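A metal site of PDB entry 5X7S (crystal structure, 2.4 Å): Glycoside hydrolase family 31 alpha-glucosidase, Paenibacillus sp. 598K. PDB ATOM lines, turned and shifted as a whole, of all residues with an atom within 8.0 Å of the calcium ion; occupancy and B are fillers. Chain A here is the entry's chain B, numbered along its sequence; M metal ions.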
ATOM      1  N   THR A 562      16.811 -10.150 -23.820  1.00  0.00           N
ATOM      2  CA  THR A 562      18.219 -10.492 -23.673  1.00  0.00           C
ATOM      3  C   THR A 562      19.035  -9.509 -24.516  1.00  0.00           C
ATOM      4  O   THR A 562      20.044  -8.941 -24.043  1.00  0.00           O
ATOM      5  CB  THR A 562      18.538 -11.913 -24.094  1.00  0.00           C
ATOM      6  OG1 THR A 562      17.847 -12.834 -23.232  1.00  0.00           O
ATOM      7  CG2 THR A 562      20.057 -12.152 -23.959  1.00  0.00           C
ATOM      8  N   ASP A 666      22.759 -19.811 -22.569  1.00  0.00           N
ATOM      9  CA  ASP A 666      21.385 -19.475 -22.192  1.00  0.00           C
ATOM     10  C   ASP A 666      21.167 -17.967 -22.034  1.00  0.00           C
ATOM     11  O   ASP A 666      20.169 -17.436 -22.516  1.00  0.00           O
ATOM     12  CB  ASP A 666      20.913 -20.216 -20.949  1.00  0.00           C
ATOM     13  CG  ASP A 666      19.380 -20.056 -20.675  1.00  0.00           C
ATOM     14  OD1 ASP A 666      18.584 -19.918 -21.640  1.00  0.00           O
ATOM     15  OD2 ASP A 666      18.974 -20.053 -19.483  1.00  0.00           O
ATOM     16  N   ASN A1114      11.388 -26.970 -22.040  1.00  0.00           N
ATOM     17  CA  ASN A1114      11.286 -26.022 -23.154  1.00  0.00           C
ATOM     18  C   ASN A1114      10.174 -24.996 -22.929  1.00  0.00           C
ATOM     19  O   ASN A1114       9.460 -24.643 -23.870  1.00  0.00           O
ATOM     20  CB  ASN A1114      11.080 -26.805 -24.475  1.00  0.00           C
ATOM     21  CG  ASN A1114      11.374 -25.979 -25.752  1.00  0.00           C
ATOM     22  OD1 ASN A1114      12.253 -25.085 -25.768  1.00  0.00           O
ATOM     23  ND2 ASN A1114      10.637 -26.293 -26.859  1.00  0.00           N
ATOM     24  N   GLY A1115      10.020 -24.538 -21.696  1.00  0.00           N
ATOM     25  CA  GLY A1115       9.071 -23.448 -21.377  1.00  0.00           C
ATOM     26  C   GLY A1115       9.416 -22.081 -21.952  1.00  0.00           C
ATOM     27  O   GLY A1115       8.539 -21.196 -21.999  1.00  0.00           O
ATOM     28  N   ASP A1116      10.693 -21.908 -22.345  1.00  0.00           N
ATOM     29  CA  ASP A1116      11.185 -20.692 -23.034  1.00  0.00           C
ATOM     30  C   ASP A1116      11.224 -20.829 -24.562  1.00  0.00           C
ATOM     31  O   ASP A1116      11.525 -19.867 -25.276  1.00  0.00           O
ATOM     32  CB  ASP A1116      12.560 -20.263 -22.512  1.00  0.00           C
ATOM     33  CG  ASP A1116      13.588 -21.357 -22.590  1.00  0.00           C
ATOM     34  OD1 ASP A1116      13.306 -22.412 -23.214  1.00  0.00           O
ATOM     35  OD2 ASP A1116      14.696 -21.136 -22.034  1.00  0.00           O
ATOM     36  N   PHE A1117      10.877 -22.025 -25.057  1.00  0.00           N
ATOM     37  CA  PHE A1117      10.741 -22.329 -26.473  1.00  0.00           C
ATOM     38  C   PHE A1117      12.074 -22.142 -27.234  1.00  0.00           C
ATOM     39  O   PHE A1117      12.085 -21.916 -28.444  1.00  0.00           O
ATOM     40  CB  PHE A1117       9.609 -21.539 -27.160  1.00  0.00           C
ATOM     41  CG  PHE A1117       8.268 -21.705 -26.519  1.00  0.00           C
ATOM     42  CD1 PHE A1117       7.553 -22.866 -26.684  1.00  0.00           C
ATOM     43  CD2 PHE A1117       7.713 -20.675 -25.757  1.00  0.00           C
ATOM     44  CE1 PHE A1117       6.315 -23.001 -26.085  1.00  0.00           C
ATOM     45  CE2 PHE A1117       6.471 -20.807 -25.178  1.00  0.00           C
ATOM     46  CZ  PHE A1117       5.763 -21.995 -25.317  1.00  0.00           C
ATOM     47  N   GLU A1118      13.180 -22.304 -26.510  1.00  0.00           N
ATOM     48  CA  GLU A1118      14.537 -22.073 -27.019  1.00  0.00           C
ATOM     49  C   GLU A1118      15.129 -23.267 -27.723  1.00  0.00           C
ATOM     50  O   GLU A1118      16.085 -23.116 -28.467  1.00  0.00           O
ATOM     51  CB  GLU A1118      15.484 -21.638 -25.894  1.00  0.00           C
ATOM     52  CG  GLU A1118      15.146 -20.269 -25.352  1.00  0.00           C
ATOM     53  CD  GLU A1118      15.172 -19.184 -26.403  1.00  0.00           C
ATOM     54  OE1 GLU A1118      16.131 -19.121 -27.193  1.00  0.00           O
ATOM     55  OE2 GLU A1118      14.218 -18.384 -26.465  1.00  0.00           O
ATOM     56  N   ARG A1119      14.572 -24.443 -27.492  1.00  0.00           N
ATOM     57  CA  ARG A1119      15.028 -25.603 -28.239  1.00  0.00           C
ATOM     58  C   ARG A1119      14.935 -25.336 -29.781  1.00  0.00           C
ATOM     59  O   ARG A1119      14.003 -24.646 -30.317  1.00  0.00           O
ATOM     60  CB  ARG A1119      14.265 -26.857 -27.831  1.00  0.00           C
ATOM     61  CG  ARG A1119      14.875 -28.191 -28.292  1.00  0.00           C
ATOM     62  CD  ARG A1119      14.363 -29.391 -27.479  1.00  0.00           C
ATOM     63  NE  ARG A1119      14.576 -29.146 -26.061  1.00  0.00           N
ATOM     64  CZ  ARG A1119      13.893 -29.658 -25.040  1.00  0.00           C
ATOM     65  NH1 ARG A1119      12.905 -30.524 -25.253  1.00  0.00           N
ATOM     66  NH2 ARG A1119      14.195 -29.270 -23.788  1.00  0.00           N
ATOM     67  N   ILE A1141       6.881 -21.930 -33.655  1.00  0.00           N
ATOM     68  CA  ILE A1141       7.964 -21.319 -32.912  1.00  0.00           C
ATOM     69  C   ILE A1141       8.988 -20.747 -33.886  1.00  0.00           C
ATOM     70  O   ILE A1141       9.480 -21.456 -34.756  1.00  0.00           O
ATOM     71  CB  ILE A1141       8.630 -22.344 -31.997  1.00  0.00           C
ATOM     72  CG1 ILE A1141       7.624 -22.860 -30.977  1.00  0.00           C
ATOM     73  CG2 ILE A1141       9.802 -21.720 -31.244  1.00  0.00           C
ATOM     74  CD1 ILE A1141       8.039 -24.154 -30.314  1.00  0.00           C
ATOM     75  N   ASP A1142       9.274 -19.452 -33.746  1.00  0.00           N
ATOM     76  CA  ASP A1142      10.420 -18.807 -34.415  1.00  0.00           C
ATOM     77  C   ASP A1142      10.857 -17.512 -33.613  1.00  0.00           C
ATOM     78  O   ASP A1142      10.445 -17.317 -32.461  1.00  0.00           O
ATOM     79  CB  ASP A1142      10.151 -18.612 -35.945  1.00  0.00           C
ATOM     80  CG  ASP A1142       9.216 -17.457 -36.257  1.00  0.00           C
ATOM     81  OD1 ASP A1142       9.004 -16.568 -35.408  1.00  0.00           O
ATOM     82  OD2 ASP A1142       8.703 -17.398 -37.401  1.00  0.00           O
ATOM     83  N   GLY A1152       9.881  -9.677 -31.518  1.00  0.00           N
ATOM     84  CA  GLY A1152      10.871 -10.603 -31.005  1.00  0.00           C
ATOM     85  C   GLY A1152      10.365 -11.404 -29.815  1.00  0.00           C
ATOM     86  O   GLY A1152       9.190 -11.370 -29.466  1.00  0.00           O
ATOM     87  N   PRO A1153      11.268 -12.151 -29.187  1.00  0.00           N
ATOM     88  CA  PRO A1153      10.908 -12.941 -28.022  1.00  0.00           C
ATOM     89  C   PRO A1153      10.866 -12.095 -26.774  1.00  0.00           C
ATOM     90  O   PRO A1153      11.211 -10.905 -26.834  1.00  0.00           O
ATOM     91  CB  PRO A1153      12.039 -13.968 -27.949  1.00  0.00           C
ATOM     92  CG  PRO A1153      13.211 -13.303 -28.600  1.00  0.00           C
ATOM     93  CD  PRO A1153      12.671 -12.344 -29.600  1.00  0.00           C
ATOM     94  N   ALA A1154      10.403 -12.691 -25.666  1.00  0.00           N
ATOM     95  CA  ALA A1154      10.493 -12.030 -24.357  1.00  0.00           C
ATOM     96  C   ALA A1154      11.933 -12.117 -23.832  1.00  0.00           C
ATOM     97  O   ALA A1154      12.469 -11.096 -23.362  1.00  0.00           O
ATOM     98  CB  ALA A1154       9.523 -12.650 -23.363  1.00  0.00           C
ATOM     99  N   ARG A1155      12.547 -13.302 -23.965  1.00  0.00           N
ATOM    100  CA  ARG A1155      13.907 -13.546 -23.539  1.00  0.00           C
ATOM    101  C   ARG A1155      14.593 -14.449 -24.565  1.00  0.00           C
ATOM    102  O   ARG A1155      13.979 -15.352 -25.120  1.00  0.00           O
ATOM    103  CB  ARG A1155      13.941 -14.232 -22.155  1.00  0.00           C
ATOM    104  CG  ARG A1155      15.270 -14.190 -21.382  1.00  0.00           C
ATOM    105  CD  ARG A1155      15.353 -15.144 -20.180  1.00  0.00           C
ATOM    106  NE  ARG A1155      15.440 -16.522 -20.638  1.00  0.00           N
ATOM    107  CZ  ARG A1155      16.539 -17.110 -21.154  1.00  0.00           C
ATOM    108  NH1 ARG A1155      17.735 -16.448 -21.247  1.00  0.00           N
ATOM    109  NH2 ARG A1155      16.467 -18.370 -21.594  1.00  0.00           N
ATOM    110  N   ARG A1156      15.877 -14.187 -24.778  1.00  0.00           N
ATOM    111  CA  ARG A1156      16.734 -14.999 -25.655  1.00  0.00           C
ATOM    112  C   ARG A1156      16.278 -14.974 -27.133  1.00  0.00           C
ATOM    113  O   ARG A1156      16.056 -13.886 -27.660  1.00  0.00           O
ATOM    114  CB  ARG A1156      16.926 -16.386 -25.054  1.00  0.00           C
ATOM    115  CG  ARG A1156      18.207 -17.048 -25.545  1.00  0.00           C
ATOM    116  CD  ARG A1156      18.417 -18.411 -24.924  1.00  0.00           C
ATOM    117  NE  ARG A1156      19.644 -18.993 -25.408  1.00  0.00           N
ATOM    118  CZ  ARG A1156      19.778 -19.701 -26.532  1.00  0.00           C
ATOM    119  NH1 ARG A1156      18.721 -19.968 -27.318  1.00  0.00           N
ATOM    120  NH2 ARG A1156      20.991 -20.140 -26.874  1.00  0.00           N
ATOM    121  N   ASN A1157      16.111 -16.125 -27.803  1.00  0.00           N
ATOM    122  CA  ASN A1157      16.034 -16.123 -29.246  1.00  0.00           C
ATOM    123  C   ASN A1157      14.719 -16.486 -29.888  1.00  0.00           C
ATOM    124  O   ASN A1157      14.560 -16.324 -31.107  1.00  0.00           O
ATOM    125  CB  ASN A1157      17.072 -17.123 -29.803  1.00  0.00           C
ATOM    126  CG  ASN A1157      17.611 -16.705 -31.169  1.00  0.00           C
ATOM    127  OD1 ASN A1157      17.733 -15.512 -31.454  1.00  0.00           O
ATOM    128  ND2 ASN A1157      17.903 -17.697 -32.014  1.00  0.00           N
ATOM    129  N   GLN A1158      13.769 -16.985 -29.099  1.00  0.00           N
ATOM    130  CA  GLN A1158      12.606 -17.666 -29.645  1.00  0.00           C
ATOM    131  C   GLN A1158      11.374 -17.531 -28.741  1.00  0.00           C
ATOM    132  O   GLN A1158      11.488 -17.419 -27.508  1.00  0.00           O
ATOM    133  CB  GLN A1158      12.938 -19.156 -29.902  1.00  0.00           C
ATOM    134  CG  GLN A1158      13.439 -19.426 -31.309  1.00  0.00           C
ATOM    135  CD  GLN A1158      13.854 -20.887 -31.594  1.00  0.00           C
ATOM    136  OE1 GLN A1158      14.195 -21.182 -32.723  1.00  0.00           O
ATOM    137  NE2 GLN A1158      13.900 -21.760 -30.578  1.00  0.00           N
ATOM    138  N   ARG A1159      10.218 -17.559 -29.390  1.00  0.00           N
ATOM    139  CA  ARG A1159       8.929 -17.508 -28.716  1.00  0.00           C
ATOM    140  C   ARG A1159       7.920 -18.249 -29.541  1.00  0.00           C
ATOM    141  O   ARG A1159       8.071 -18.365 -30.728  1.00  0.00           O
ATOM    142  CB  ARG A1159       8.467 -16.070 -28.434  1.00  0.00           C
ATOM    143  CG  ARG A1159       7.906 -15.270 -29.590  1.00  0.00           C
ATOM    144  CD  ARG A1159       8.941 -14.790 -30.613  1.00  0.00           C
ATOM    145  NE  ARG A1159       8.341 -13.901 -31.630  1.00  0.00           N
ATOM    146  CZ  ARG A1159       7.579 -14.307 -32.651  1.00  0.00           C
ATOM    147  NH1 ARG A1159       7.302 -15.593 -32.844  1.00  0.00           N
ATOM    148  NH2 ARG A1159       7.109 -13.419 -33.513  1.00  0.00           N
ATOM    149  N   ALA A1160       6.885 -18.778 -28.902  1.00  0.00           N
ATOM    150  CA  ALA A1160       5.835 -19.470 -29.645  1.00  0.00           C
ATOM    151  C   ALA A1160       4.832 -18.422 -30.051  1.00  0.00           C
ATOM    152  O   ALA A1160       4.688 -17.392 -29.364  1.00  0.00           O
ATOM    153  CB  ALA A1160       5.194 -20.536 -28.778  1.00  0.00           C
ATOM    154  N   TRP A1223       4.219  -7.170 -24.486  1.00  0.00           N
ATOM    155  CA  TRP A1223       4.531  -8.253 -23.521  1.00  0.00           C
ATOM    156  C   TRP A1223       3.975  -7.915 -22.099  1.00  0.00           C
ATOM    157  O   TRP A1223       4.235  -6.858 -21.542  1.00  0.00           O
ATOM    158  CB  TRP A1223       6.054  -8.537 -23.415  1.00  0.00           C
ATOM    159  CG  TRP A1223       6.682  -9.296 -24.569  1.00  0.00           C
ATOM    160  CD1 TRP A1223       7.661  -8.842 -25.415  1.00  0.00           C
ATOM    161  CD2 TRP A1223       6.438 -10.666 -24.962  1.00  0.00           C
ATOM    162  NE1 TRP A1223       8.017  -9.828 -26.317  1.00  0.00           N
ATOM    163  CE2 TRP A1223       7.275 -10.951 -26.061  1.00  0.00           C
ATOM    164  CE3 TRP A1223       5.570 -11.663 -24.496  1.00  0.00           C
ATOM    165  CZ2 TRP A1223       7.279 -12.195 -26.674  1.00  0.00           C
ATOM    166  CZ3 TRP A1223       5.578 -12.898 -25.109  1.00  0.00           C
ATOM    167  CH2 TRP A1223       6.420 -13.164 -26.185  1.00  0.00           C
ATOM    168  N   ILE A1254       3.857 -16.210 -26.906  1.00  0.00           N
ATOM    169  CA  ILE A1254       4.021 -16.810 -25.594  1.00  0.00           C
ATOM    170  C   ILE A1254       5.502 -17.155 -25.394  1.00  0.00           C
ATOM    171  O   ILE A1254       6.121 -17.814 -26.226  1.00  0.00           O
ATOM    172  CB  ILE A1254       3.250 -18.133 -25.499  1.00  0.00           C
ATOM    173  CG1 ILE A1254       1.784 -17.960 -25.941  1.00  0.00           C
ATOM    174  CG2 ILE A1254       3.254 -18.663 -24.072  1.00  0.00           C
ATOM    175  CD1 ILE A1254       1.021 -19.247 -26.009  1.00  0.00           C
ATOM    176  N   ASP A1255       6.029 -16.757 -24.240  1.00  0.00           N
ATOM    177  CA  ASP A1255       7.394 -17.045 -23.875  1.00  0.00           C
ATOM    178  C   ASP A1255       7.670 -17.188 -22.328  1.00  0.00           C
ATOM    179  O   ASP A1255       6.885 -16.772 -21.493  1.00  0.00           O
ATOM    180  CB  ASP A1255       8.294 -15.946 -24.490  1.00  0.00           C
ATOM    181  CG  ASP A1255       9.683 -16.396 -24.701  1.00  0.00           C
ATOM    182  OD1 ASP A1255       9.942 -17.588 -24.441  1.00  0.00           O
ATOM    183  OD2 ASP A1255      10.529 -15.612 -25.113  1.00  0.00           O
ATOM    184  N   GLU A1256       8.789 -17.813 -21.976  1.00  0.00           N
ATOM    185  CA  GLU A1256       9.277 -17.881 -20.617  1.00  0.00           C
ATOM    186  C   GLU A1256       8.222 -18.438 -19.654  1.00  0.00           C
ATOM    187  O   GLU A1256       7.932 -17.853 -18.626  1.00  0.00           O
ATOM    188  CB  GLU A1256       9.782 -16.492 -20.152  1.00  0.00           C
ATOM    189  CG  GLU A1256      10.803 -15.833 -21.080  1.00  0.00           C
ATOM    190  CD  GLU A1256      11.948 -16.757 -21.484  1.00  0.00           C
ATOM    191  OE1 GLU A1256      12.751 -17.081 -20.625  1.00  0.00           O
ATOM    192  OE2 GLU A1256      12.091 -17.145 -22.672  1.00  0.00           O
ATOM    193  N   VAL A1257       7.669 -19.587 -20.036  1.00  0.00           N
ATOM    194  CA  VAL A1257       6.687 -20.304 -19.222  1.00  0.00           C
ATOM    195  C   VAL A1257       7.446 -21.037 -18.147  1.00  0.00           C
ATOM    196  O   VAL A1257       8.383 -21.780 -18.458  1.00  0.00           O
ATOM    197  CB  VAL A1257       5.893 -21.320 -20.064  1.00  0.00           C
ATOM    198  CG1 VAL A1257       4.675 -21.836 -19.303  1.00  0.00           C
ATOM    199  CG2 VAL A1257       5.416 -20.687 -21.364  1.00  0.00           C
HETATM  200 CA    CA M   1      12.252 -17.531 -25.328  1.00  0.00          CA
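The side-chain amide nitrogen of Gln 1158 is in hydrogen-bond range of the backbone carbonyl oxygen of Phe 1117.
NE2 of Gln 1158 sits at hydrogen-bond distance from O of Arg 1119, at 2.9 Å.
OE1 of Glu 1118 is in hydrogen-bond range of N of Asn 1157 (3.1 Å).
OE1 of Glu 1118 is in salt-bridge range of NH1 of Arg 1156, 2.7 Å away.
The backbone NH (N) of Glu 1118 is in hydrogen-bond range of the side-chain amide oxygen (OD1) of Asn 1114 (3.0 Å).
N of Ala 1154 sits close to OD2 of Asp 1255 (3.0 Å).
The backbone NH of Glu 1256 lies within hydrogen-bond range of the backbone carbonyl oxygen of Gly 1115, 3.4 Å away.
OD1 of Asp 666 is in salt-bridge range of NH2 of Arg 1155, 2.6 Å away.
Within 4 Å of the calcium ion: Asp 1116, Glu 1118, Arg 1155, Gln 1158, Asp 1255 and Glu 1256.
Along chain A the residues within 4 Å of the calcium ion span positions 1116 to 1256.
The nearest printed residue that does not touch the calcium ion is Pro 1153 (4.4 Å).
O of Gln 1158 binds the calcium ion (2.3 Å).
The calcium ion is bound by OE2 of Glu 1118.
O of Asp 1116 is bound to the calcium ion.
The calcium ion is bound by OD1 of Asp 1255, 2.5 Å away.
The calcium ion is bound by OD2 of Asp 1255 (2.6 Å).
OE2 of Glu 1256 is bound to the calcium ion (2.7 Å).
The calcium ion is bound by O of Arg 1155, 2.8 Å away.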
